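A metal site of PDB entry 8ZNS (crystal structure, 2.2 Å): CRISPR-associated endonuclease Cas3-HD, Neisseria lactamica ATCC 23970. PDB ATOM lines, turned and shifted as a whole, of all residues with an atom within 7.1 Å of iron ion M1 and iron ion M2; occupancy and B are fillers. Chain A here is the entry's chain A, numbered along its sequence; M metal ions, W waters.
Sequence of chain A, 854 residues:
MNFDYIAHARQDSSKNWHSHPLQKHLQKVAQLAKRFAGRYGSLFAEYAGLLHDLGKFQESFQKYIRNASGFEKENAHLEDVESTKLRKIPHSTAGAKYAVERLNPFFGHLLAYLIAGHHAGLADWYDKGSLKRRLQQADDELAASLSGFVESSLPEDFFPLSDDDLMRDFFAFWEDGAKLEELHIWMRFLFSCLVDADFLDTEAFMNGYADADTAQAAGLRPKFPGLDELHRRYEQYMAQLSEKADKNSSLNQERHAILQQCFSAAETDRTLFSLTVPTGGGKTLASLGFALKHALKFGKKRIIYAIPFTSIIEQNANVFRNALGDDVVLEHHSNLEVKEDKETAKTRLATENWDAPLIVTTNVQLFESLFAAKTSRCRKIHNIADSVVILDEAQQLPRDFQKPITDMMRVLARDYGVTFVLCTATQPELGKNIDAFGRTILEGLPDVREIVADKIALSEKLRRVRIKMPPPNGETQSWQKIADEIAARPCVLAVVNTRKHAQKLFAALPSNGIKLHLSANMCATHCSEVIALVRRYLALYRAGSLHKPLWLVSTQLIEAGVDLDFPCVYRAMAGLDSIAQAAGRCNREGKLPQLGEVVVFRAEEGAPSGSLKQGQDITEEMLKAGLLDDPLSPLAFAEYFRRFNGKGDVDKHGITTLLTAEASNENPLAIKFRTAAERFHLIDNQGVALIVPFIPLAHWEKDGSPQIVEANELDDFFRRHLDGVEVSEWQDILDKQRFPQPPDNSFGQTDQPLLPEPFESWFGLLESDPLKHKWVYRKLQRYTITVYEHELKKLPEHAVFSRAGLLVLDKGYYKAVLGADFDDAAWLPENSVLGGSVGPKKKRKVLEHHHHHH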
ATOM      1  N   ALA A   7     -22.828  18.262 -15.075  1.00  0.00           N
ATOM      2  CA  ALA A   7     -22.778  19.698 -14.815  1.00  0.00           C
ATOM      3  C   ALA A   7     -21.490  20.350 -15.280  1.00  0.00           C
ATOM      4  O   ALA A   7     -21.516  21.507 -15.679  1.00  0.00           O
ATOM      5  CB  ALA A   7     -22.959  19.979 -13.315  1.00  0.00           C
ATOM      6  N   HIS A   8     -20.376  19.617 -15.237  1.00  0.00           N
ATOM      7  CA  HIS A   8     -19.065  20.124 -15.617  1.00  0.00           C
ATOM      8  C   HIS A   8     -18.221  18.988 -16.192  1.00  0.00           C
ATOM      9  O   HIS A   8     -18.455  17.806 -15.907  1.00  0.00           O
ATOM     10  CB  HIS A   8     -18.280  20.737 -14.426  1.00  0.00           C
ATOM     11  CG  HIS A   8     -19.083  21.674 -13.572  1.00  0.00           C
ATOM     12  ND1 HIS A   8     -19.717  21.267 -12.415  1.00  0.00           N
ATOM     13  CD2 HIS A   8     -19.335  23.002 -13.691  1.00  0.00           C
ATOM     14  CE1 HIS A   8     -20.334  22.302 -11.869  1.00  0.00           C
ATOM     15  NE2 HIS A   8     -20.120  23.361 -12.630  1.00  0.00           N
ATOM     16  N   HIS A  20     -18.753  15.778 -13.787  1.00  0.00           N
ATOM     17  CA  HIS A  20     -19.443  16.051 -12.530  1.00  0.00           C
ATOM     18  C   HIS A  20     -20.925  15.729 -12.677  1.00  0.00           C
ATOM     19  O   HIS A  20     -21.606  16.394 -13.465  1.00  0.00           O
ATOM     20  CB  HIS A  20     -19.233  17.520 -12.179  1.00  0.00           C
ATOM     21  CG  HIS A  20     -19.490  17.885 -10.755  1.00  0.00           C
ATOM     22  ND1 HIS A  20     -19.606  19.193 -10.347  1.00  0.00           N
ATOM     23  CD2 HIS A  20     -19.655  17.126  -9.641  1.00  0.00           C
ATOM     24  CE1 HIS A  20     -19.824  19.231  -9.041  1.00  0.00           C
ATOM     25  NE2 HIS A  20     -19.871  17.994  -8.596  1.00  0.00           N
ATOM     26  N   LEU A  22     -24.815  15.779 -12.665  1.00  0.00           N
ATOM     27  CA  LEU A  22     -25.665  16.953 -12.474  1.00  0.00           C
ATOM     28  C   LEU A  22     -26.560  16.807 -11.240  1.00  0.00           C
ATOM     29  O   LEU A  22     -26.672  17.737 -10.431  1.00  0.00           O
ATOM     30  CB  LEU A  22     -26.508  17.203 -13.738  1.00  0.00           C
ATOM     31  CG  LEU A  22     -27.568  18.326 -13.722  1.00  0.00           C
ATOM     32  CD1 LEU A  22     -26.961  19.706 -13.315  1.00  0.00           C
ATOM     33  CD2 LEU A  22     -28.305  18.434 -15.056  1.00  0.00           C
ATOM     34  N   HIS A  25     -24.621  17.367  -8.029  1.00  0.00           N
ATOM     35  CA  HIS A  25     -24.202  18.749  -7.857  1.00  0.00           C
ATOM     36  C   HIS A  25     -25.385  19.615  -7.418  1.00  0.00           C
ATOM     37  O   HIS A  25     -25.232  20.449  -6.511  1.00  0.00           O
ATOM     38  CB  HIS A  25     -23.585  19.234  -9.174  1.00  0.00           C
ATOM     39  CG  HIS A  25     -23.342  20.709  -9.248  1.00  0.00           C
ATOM     40  ND1 HIS A  25     -22.293  21.333  -8.615  1.00  0.00           N
ATOM     41  CD2 HIS A  25     -24.012  21.677  -9.923  1.00  0.00           C
ATOM     42  CE1 HIS A  25     -22.335  22.625  -8.880  1.00  0.00           C
ATOM     43  NE2 HIS A  25     -23.361  22.856  -9.669  1.00  0.00           N
ATOM     44  N   LEU A  26     -26.569  19.408  -8.016  1.00  0.00           N
ATOM     45  CA  LEU A  26     -27.736  20.166  -7.593  1.00  0.00           C
ATOM     46  C   LEU A  26     -28.066  19.883  -6.136  1.00  0.00           C
ATOM     47  O   LEU A  26     -28.399  20.806  -5.371  1.00  0.00           O
ATOM     48  CB  LEU A  26     -28.941  19.873  -8.498  1.00  0.00           C
ATOM     49  CG  LEU A  26     -28.912  20.394  -9.941  1.00  0.00           C
ATOM     50  CD1 LEU A  26     -30.165  19.890 -10.715  1.00  0.00           C
ATOM     51  CD2 LEU A  26     -28.817  21.898  -9.981  1.00  0.00           C
ATOM     52  N   VAL A  29     -25.193  21.474  -3.873  1.00  0.00           N
ATOM     53  CA  VAL A  29     -25.221  22.928  -3.855  1.00  0.00           C
ATOM     54  C   VAL A  29     -26.430  23.415  -3.072  1.00  0.00           C
ATOM     55  O   VAL A  29     -26.311  24.364  -2.291  1.00  0.00           O
ATOM     56  CB  VAL A  29     -25.191  23.484  -5.292  1.00  0.00           C
ATOM     57  CG1 VAL A  29     -25.558  24.970  -5.327  1.00  0.00           C
ATOM     58  CG2 VAL A  29     -23.804  23.263  -5.868  1.00  0.00           C
ATOM     59  N   GLY A  49     -30.219  26.796  -4.779  1.00  0.00           N
ATOM     60  CA  GLY A  49     -29.171  25.834  -5.121  1.00  0.00           C
ATOM     61  C   GLY A  49     -29.717  24.679  -5.943  1.00  0.00           C
ATOM     62  O   GLY A  49     -29.057  24.203  -6.885  1.00  0.00           O
ATOM     63  N   HIS A  52     -30.547  26.188  -9.600  1.00  0.00           N
ATOM     64  CA  HIS A  52     -29.649  27.082 -10.334  1.00  0.00           C
ATOM     65  C   HIS A  52     -29.201  26.467 -11.667  1.00  0.00           C
ATOM     66  O   HIS A  52     -29.240  27.146 -12.700  1.00  0.00           O
ATOM     67  CB  HIS A  52     -28.450  27.480  -9.442  1.00  0.00           C
ATOM     68  CG  HIS A  52     -27.315  26.497  -9.436  1.00  0.00           C
ATOM     69  ND1 HIS A  52     -27.373  25.286  -8.765  1.00  0.00           N
ATOM     70  CD2 HIS A  52     -26.078  26.551  -9.998  1.00  0.00           C
ATOM     71  CE1 HIS A  52     -26.234  24.649  -8.932  1.00  0.00           C
ATOM     72  NE2 HIS A  52     -25.432  25.375  -9.687  1.00  0.00           N
ATOM     73  N   ASP A  53     -28.858  25.171 -11.677  1.00  0.00           N
ATOM     74  CA  ASP A  53     -28.402  24.519 -12.909  1.00  0.00           C
ATOM     75  C   ASP A  53     -29.489  23.660 -13.565  1.00  0.00           C
ATOM     76  O   ASP A  53     -29.178  22.699 -14.286  1.00  0.00           O
ATOM     77  CB  ASP A  53     -27.134  23.671 -12.654  1.00  0.00           C
ATOM     78  CG  ASP A  53     -25.833  24.504 -12.605  1.00  0.00           C
ATOM     79  OD1 ASP A  53     -25.807  25.694 -13.012  1.00  0.00           O
ATOM     80  OD2 ASP A  53     -24.816  23.953 -12.132  1.00  0.00           O
ATOM     81  N   LYS A  56     -29.160  22.877 -17.318  1.00  0.00           N
ATOM     82  CA  LYS A  56     -28.228  21.955 -17.939  1.00  0.00           C
ATOM     83  C   LYS A  56     -28.894  20.628 -18.314  1.00  0.00           C
ATOM     84  O   LYS A  56     -28.268  19.820 -18.992  1.00  0.00           O
ATOM     85  CB  LYS A  56     -27.023  21.716 -17.029  1.00  0.00           C
ATOM     86  CG  LYS A  56     -26.129  22.931 -16.880  1.00  0.00           C
ATOM     87  CD  LYS A  56     -25.045  22.691 -15.801  1.00  0.00           C
ATOM     88  CE  LYS A  56     -24.062  23.870 -15.749  1.00  0.00           C
ATOM     89  NZ  LYS A  56     -23.220  23.881 -14.506  1.00  0.00           N
ATOM     90  N   HIS A  77     -20.004  25.581 -19.192  1.00  0.00           N
ATOM     91  CA  HIS A  77     -20.960  26.159 -18.264  1.00  0.00           C
ATOM     92  C   HIS A  77     -20.826  27.683 -18.149  1.00  0.00           C
ATOM     93  O   HIS A  77     -21.689  28.306 -17.527  1.00  0.00           O
ATOM     94  CB  HIS A  77     -20.793  25.521 -16.892  1.00  0.00           C
ATOM     95  CG  HIS A  77     -19.384  25.560 -16.370  1.00  0.00           C
ATOM     96  ND1 HIS A  77     -18.329  24.999 -17.051  1.00  0.00           N
ATOM     97  CD2 HIS A  77     -18.862  26.108 -15.248  1.00  0.00           C
ATOM     98  CE1 HIS A  77     -17.206  25.198 -16.368  1.00  0.00           C
ATOM     99  NE2 HIS A  77     -17.510  25.866 -15.278  1.00  0.00           N
ATOM    100  N   LEU A  78     -19.780  28.290 -18.706  1.00  0.00           N
ATOM    101  CA  LEU A  78     -19.608  29.748 -18.609  1.00  0.00           C
ATOM    102  C   LEU A  78     -20.426  30.431 -19.696  1.00  0.00           C
ATOM    103  O   LEU A  78     -19.905  30.805 -20.753  1.00  0.00           O
ATOM    104  CB  LEU A  78     -18.123  30.121 -18.712  1.00  0.00           C
ATOM    105  CG  LEU A  78     -17.268  29.927 -17.452  1.00  0.00           C
ATOM    106  CD1 LEU A  78     -17.133  28.451 -17.121  1.00  0.00           C
ATOM    107  CD2 LEU A  78     -15.893  30.557 -17.611  1.00  0.00           C
ATOM    108  N   GLU A  79     -21.731  30.649 -19.417  1.00  0.00           N
ATOM    109  CA  GLU A  79     -22.653  31.249 -20.394  1.00  0.00           C
ATOM    110  C   GLU A  79     -22.269  32.674 -20.804  1.00  0.00           C
ATOM    111  O   GLU A  79     -22.666  33.115 -21.891  1.00  0.00           O
ATOM    112  CB  GLU A  79     -24.109  31.229 -19.876  1.00  0.00           C
ATOM    113  CG  GLU A  79     -24.299  31.265 -18.314  1.00  0.00           C
ATOM    114  CD  GLU A  79     -25.773  31.265 -17.848  1.00  0.00           C
ATOM    115  OE1 GLU A  79     -26.166  32.175 -17.082  1.00  0.00           O
ATOM    116  OE2 GLU A  79     -26.543  30.374 -18.224  1.00  0.00           O
ATOM    117  N   HIS A  91     -28.045  28.385 -19.689  1.00  0.00           N
ATOM    118  CA  HIS A  91     -28.666  27.448 -18.766  1.00  0.00           C
ATOM    119  C   HIS A  91     -29.183  28.071 -17.470  1.00  0.00           C
ATOM    120  O   HIS A  91     -29.981  27.433 -16.783  1.00  0.00           O
ATOM    121  CB  HIS A  91     -27.668  26.324 -18.421  1.00  0.00           C
ATOM    122  CG  HIS A  91     -26.557  26.769 -17.517  1.00  0.00           C
ATOM    123  ND1 HIS A  91     -25.365  27.275 -17.997  1.00  0.00           N
ATOM    124  CD2 HIS A  91     -26.485  26.827 -16.167  1.00  0.00           C
ATOM    125  CE1 HIS A  91     -24.600  27.610 -16.976  1.00  0.00           C
ATOM    126  NE2 HIS A  91     -25.248  27.330 -15.853  1.00  0.00           N
ATOM    127  N   SER A  92     -28.800  29.314 -17.127  1.00  0.00           N
ATOM    128  CA  SER A  92     -29.171  29.848 -15.811  1.00  0.00           C
ATOM    129  C   SER A  92     -30.627  30.266 -15.734  1.00  0.00           C
ATOM    130  O   SER A  92     -31.173  30.327 -14.635  1.00  0.00           O
ATOM    131  CB  SER A  92     -28.299  31.054 -15.429  1.00  0.00           C
ATOM    132  OG  SER A  92     -28.364  32.135 -16.369  1.00  0.00           O
ATOM    133  N   ILE A 115     -31.095  32.991  -9.276  1.00  0.00           N
ATOM    134  CA  ILE A 115     -30.788  31.885 -10.181  1.00  0.00           C
ATOM    135  C   ILE A 115     -30.260  32.415 -11.501  1.00  0.00           C
ATOM    136  O   ILE A 115     -29.284  31.899 -12.050  1.00  0.00           O
ATOM    137  CB  ILE A 115     -32.019  30.997 -10.411  1.00  0.00           C
ATOM    138  CG1 ILE A 115     -32.406  30.239  -9.157  1.00  0.00           C
ATOM    139  CG2 ILE A 115     -31.737  29.994 -11.548  1.00  0.00           C
ATOM    140  CD1 ILE A 115     -33.824  29.739  -9.274  1.00  0.00           C
ATOM    141  N   HIS A 118     -26.548  33.806 -11.446  1.00  0.00           N
ATOM    142  CA  HIS A 118     -25.469  33.026 -10.841  1.00  0.00           C
ATOM    143  C   HIS A 118     -24.236  32.921 -11.750  1.00  0.00           C
ATOM    144  O   HIS A 118     -23.162  32.538 -11.272  1.00  0.00           O
ATOM    145  CB  HIS A 118     -25.992  31.651 -10.392  1.00  0.00           C
ATOM    146  CG  HIS A 118     -25.934  30.555 -11.419  1.00  0.00           C
ATOM    147  ND1 HIS A 118     -27.046  30.121 -12.111  1.00  0.00           N
ATOM    148  CD2 HIS A 118     -24.920  29.740 -11.804  1.00  0.00           C
ATOM    149  CE1 HIS A 118     -26.726  29.113 -12.900  1.00  0.00           C
ATOM    150  NE2 HIS A 118     -25.435  28.868 -12.747  1.00  0.00           N
ATOM    151  N   HIS A 119     -24.322  33.327 -13.017  1.00  0.00           N
ATOM    152  CA  HIS A 119     -23.125  33.620 -13.798  1.00  0.00           C
ATOM    153  C   HIS A 119     -22.920  35.108 -14.063  1.00  0.00           C
ATOM    154  O   HIS A 119     -21.842  35.642 -13.795  1.00  0.00           O
ATOM    155  CB  HIS A 119     -23.163  32.852 -15.139  1.00  0.00           C
ATOM    156  CG  HIS A 119     -23.037  31.373 -15.000  1.00  0.00           C
ATOM    157  ND1 HIS A 119     -21.820  30.743 -14.954  1.00  0.00           N
ATOM    158  CD2 HIS A 119     -23.974  30.401 -14.877  1.00  0.00           C
ATOM    159  CE1 HIS A 119     -22.008  29.439 -14.818  1.00  0.00           C
ATOM    160  NE2 HIS A 119     -23.307  29.212 -14.778  1.00  0.00           N
ATOM    161  N   LEU A 194     -25.593  30.964  -2.396  1.00  0.00           N
ATOM    162  CA  LEU A 194     -25.683  30.183  -3.617  1.00  0.00           C
ATOM    163  C   LEU A 194     -24.320  30.092  -4.292  1.00  0.00           C
ATOM    164  O   LEU A 194     -23.837  28.990  -4.595  1.00  0.00           O
ATOM    165  CB  LEU A 194     -26.704  30.811  -4.547  1.00  0.00           C
ATOM    166  CG  LEU A 194     -26.664  30.263  -5.956  1.00  0.00           C
ATOM    167  CD1 LEU A 194     -26.949  28.740  -5.887  1.00  0.00           C
ATOM    168  CD2 LEU A 194     -27.693  30.978  -6.848  1.00  0.00           C
ATOM    169  N   ASP A 198     -21.974  26.780  -4.777  1.00  0.00           N
ATOM    170  CA  ASP A 198     -21.760  26.334  -6.155  1.00  0.00           C
ATOM    171  C   ASP A 198     -20.272  26.195  -6.438  1.00  0.00           C
ATOM    172  O   ASP A 198     -19.797  25.130  -6.841  1.00  0.00           O
ATOM    173  CB  ASP A 198     -22.417  27.359  -7.089  1.00  0.00           C
ATOM    174  CG  ASP A 198     -22.493  26.927  -8.547  1.00  0.00           C
ATOM    175  OD1 ASP A 198     -22.524  25.713  -8.889  1.00  0.00           O
ATOM    176  OD2 ASP A 198     -22.584  27.844  -9.394  1.00  0.00           O
ATOM    177  N   PHE A 199     -19.525  27.271  -6.191  1.00  0.00           N
ATOM    178  CA  PHE A 199     -18.082  27.269  -6.460  1.00  0.00           C
ATOM    179  C   PHE A 199     -17.365  26.223  -5.624  1.00  0.00           C
ATOM    180  O   PHE A 199     -16.476  25.528  -6.122  1.00  0.00           O
ATOM    181  CB  PHE A 199     -17.483  28.664  -6.188  1.00  0.00           C
ATOM    182  CG  PHE A 199     -17.889  29.719  -7.192  1.00  0.00           C
ATOM    183  CD1 PHE A 199     -18.852  29.442  -8.167  1.00  0.00           C
ATOM    184  CD2 PHE A 199     -17.313  30.975  -7.168  1.00  0.00           C
ATOM    185  CE1 PHE A 199     -19.232  30.394  -9.103  1.00  0.00           C
ATOM    186  CE2 PHE A 199     -17.673  31.932  -8.097  1.00  0.00           C
ATOM    187  CZ  PHE A 199     -18.647  31.635  -9.078  1.00  0.00           C
ATOM    188  N   ASP A 201     -18.497  23.389  -4.346  1.00  0.00           N
ATOM    189  CA  ASP A 201     -18.771  22.047  -4.866  1.00  0.00           C
ATOM    190  C   ASP A 201     -18.001  21.784  -6.152  1.00  0.00           C
ATOM    191  O   ASP A 201     -17.408  20.704  -6.349  1.00  0.00           O
ATOM    192  CB  ASP A 201     -20.277  21.876  -5.121  1.00  0.00           C
ATOM    193  CG  ASP A 201     -20.668  20.419  -5.360  1.00  0.00           C
ATOM    194  OD1 ASP A 201     -20.533  19.626  -4.413  1.00  0.00           O
ATOM    195  OD2 ASP A 201     -21.092  20.087  -6.485  1.00  0.00           O
ATOM    196  N   THR A 202     -18.000  22.765  -7.058  1.00  0.00           N
ATOM    197  CA  THR A 202     -17.267  22.576  -8.305  1.00  0.00           C
ATOM    198  C   THR A 202     -15.774  22.415  -8.041  1.00  0.00           C
ATOM    199  O   THR A 202     -15.097  21.634  -8.706  1.00  0.00           O
ATOM    200  CB  THR A 202     -17.519  23.742  -9.258  1.00  0.00           C
ATOM    201  OG1 THR A 202     -18.921  23.966  -9.340  1.00  0.00           O
ATOM    202  CG2 THR A 202     -16.990  23.418 -10.648  1.00  0.00           C
ATOM    203  N   ARG A 348     -12.563  31.522 -12.524  1.00  0.00           N
ATOM    204  CA  ARG A 348     -13.840  31.737 -11.855  1.00  0.00           C
ATOM    205  C   ARG A 348     -13.811  31.178 -10.431  1.00  0.00           C
ATOM    206  O   ARG A 348     -14.294  31.831  -9.497  1.00  0.00           O
ATOM    207  CB  ARG A 348     -14.979  31.093 -12.656  1.00  0.00           C
ATOM    208  CG  ARG A 348     -16.388  31.505 -12.260  1.00  0.00           C
ATOM    209  CD  ARG A 348     -17.400  31.229 -13.384  1.00  0.00           C
ATOM    210  NE  ARG A 348     -18.782  31.289 -12.913  1.00  0.00           N
ATOM    211  CZ  ARG A 348     -19.454  30.230 -12.480  1.00  0.00           C
ATOM    212  NH1 ARG A 348     -18.877  29.036 -12.430  1.00  0.00           N
ATOM    213  NH2 ARG A 348     -20.713  30.367 -12.083  1.00  0.00           N
HETATM  214 FE    FE M   1     -23.505  24.815 -10.548  1.00  0.00          FE
HETATM  215 FE    FE M   2     -24.443  27.567 -13.950  1.00  0.00          FE
HETATM  216  O   HOH W   1     -22.105  26.372 -12.376  1.00  0.00           O
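The backbone carbonyl oxygen of His 118 sits at hydrogen-bond distance from the guanidinium group of Arg 348 (3.4 Å).
NZ of Lys 56 lies within hydrogen-bond range of O of Ala 7 (3.1 Å).
The side-chain hydroxyl (OG1) of Thr 202 lies within hydrogen-bond range of the backbone carbonyl oxygen (O) of Asp 198, 2.9 Å away.
A ring nitrogen (ND1) of His 119 sits at hydrogen-bond distance from the guanidinium group (NH2) of Arg 348 (3.1 Å).
NE2 of His 119 lies close to O of His 77 (3.3 Å).
A ring nitrogen (ND1) of His 52 sits at hydrogen-bond distance from the backbone carbonyl oxygen (O) of Gly 49.
The side-chain carboxylate (OD2) of Asp 53 sits close to the side-chain amino group (NZ) of Lys 56 (2.9 Å).
A ring nitrogen (ND1) of His 25 is in hydrogen-bond range of the side-chain carboxylate of Asp 201 (2.7 Å).
Within 4 Å of iron ion M1: His 25, His 52, Asp 53 and Asp 198.
The nearest printed residue that does not touch iron ion M1 is Lys 56 (4.1 Å).
Lys 56 touches iron ion M2.
The nearest printed residue that does not touch iron ion M2 is His 52 (4.4 Å).
Iron ion M1 is bound by OD1 of Asp 198, NE2 of His 25, NE2 of His 52 and OD2 of Asp 53.
Iron ion M1 has four donor atoms within binding distance.
Slightly farther from iron ion M1 lies water W1 (2.8 Å).
Iron ion M2 is bound by a ring nitrogen (NE2) of His 118 (2.0 Å), a ring nitrogen (NE2) of His 91 (2.1 Å), a ring nitrogen (NE2) of His 119 (2.2 Å) and the side-chain carboxylate (OD1) of Asp 53 (2.5 Å).
Iron ion M2 has four donor atoms within binding distance.
Water W1 bridges the side-chain carboxylate of Asp 198 (3.4 Å) and the side-chain amino group of Lys 56 (3.5 Å).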
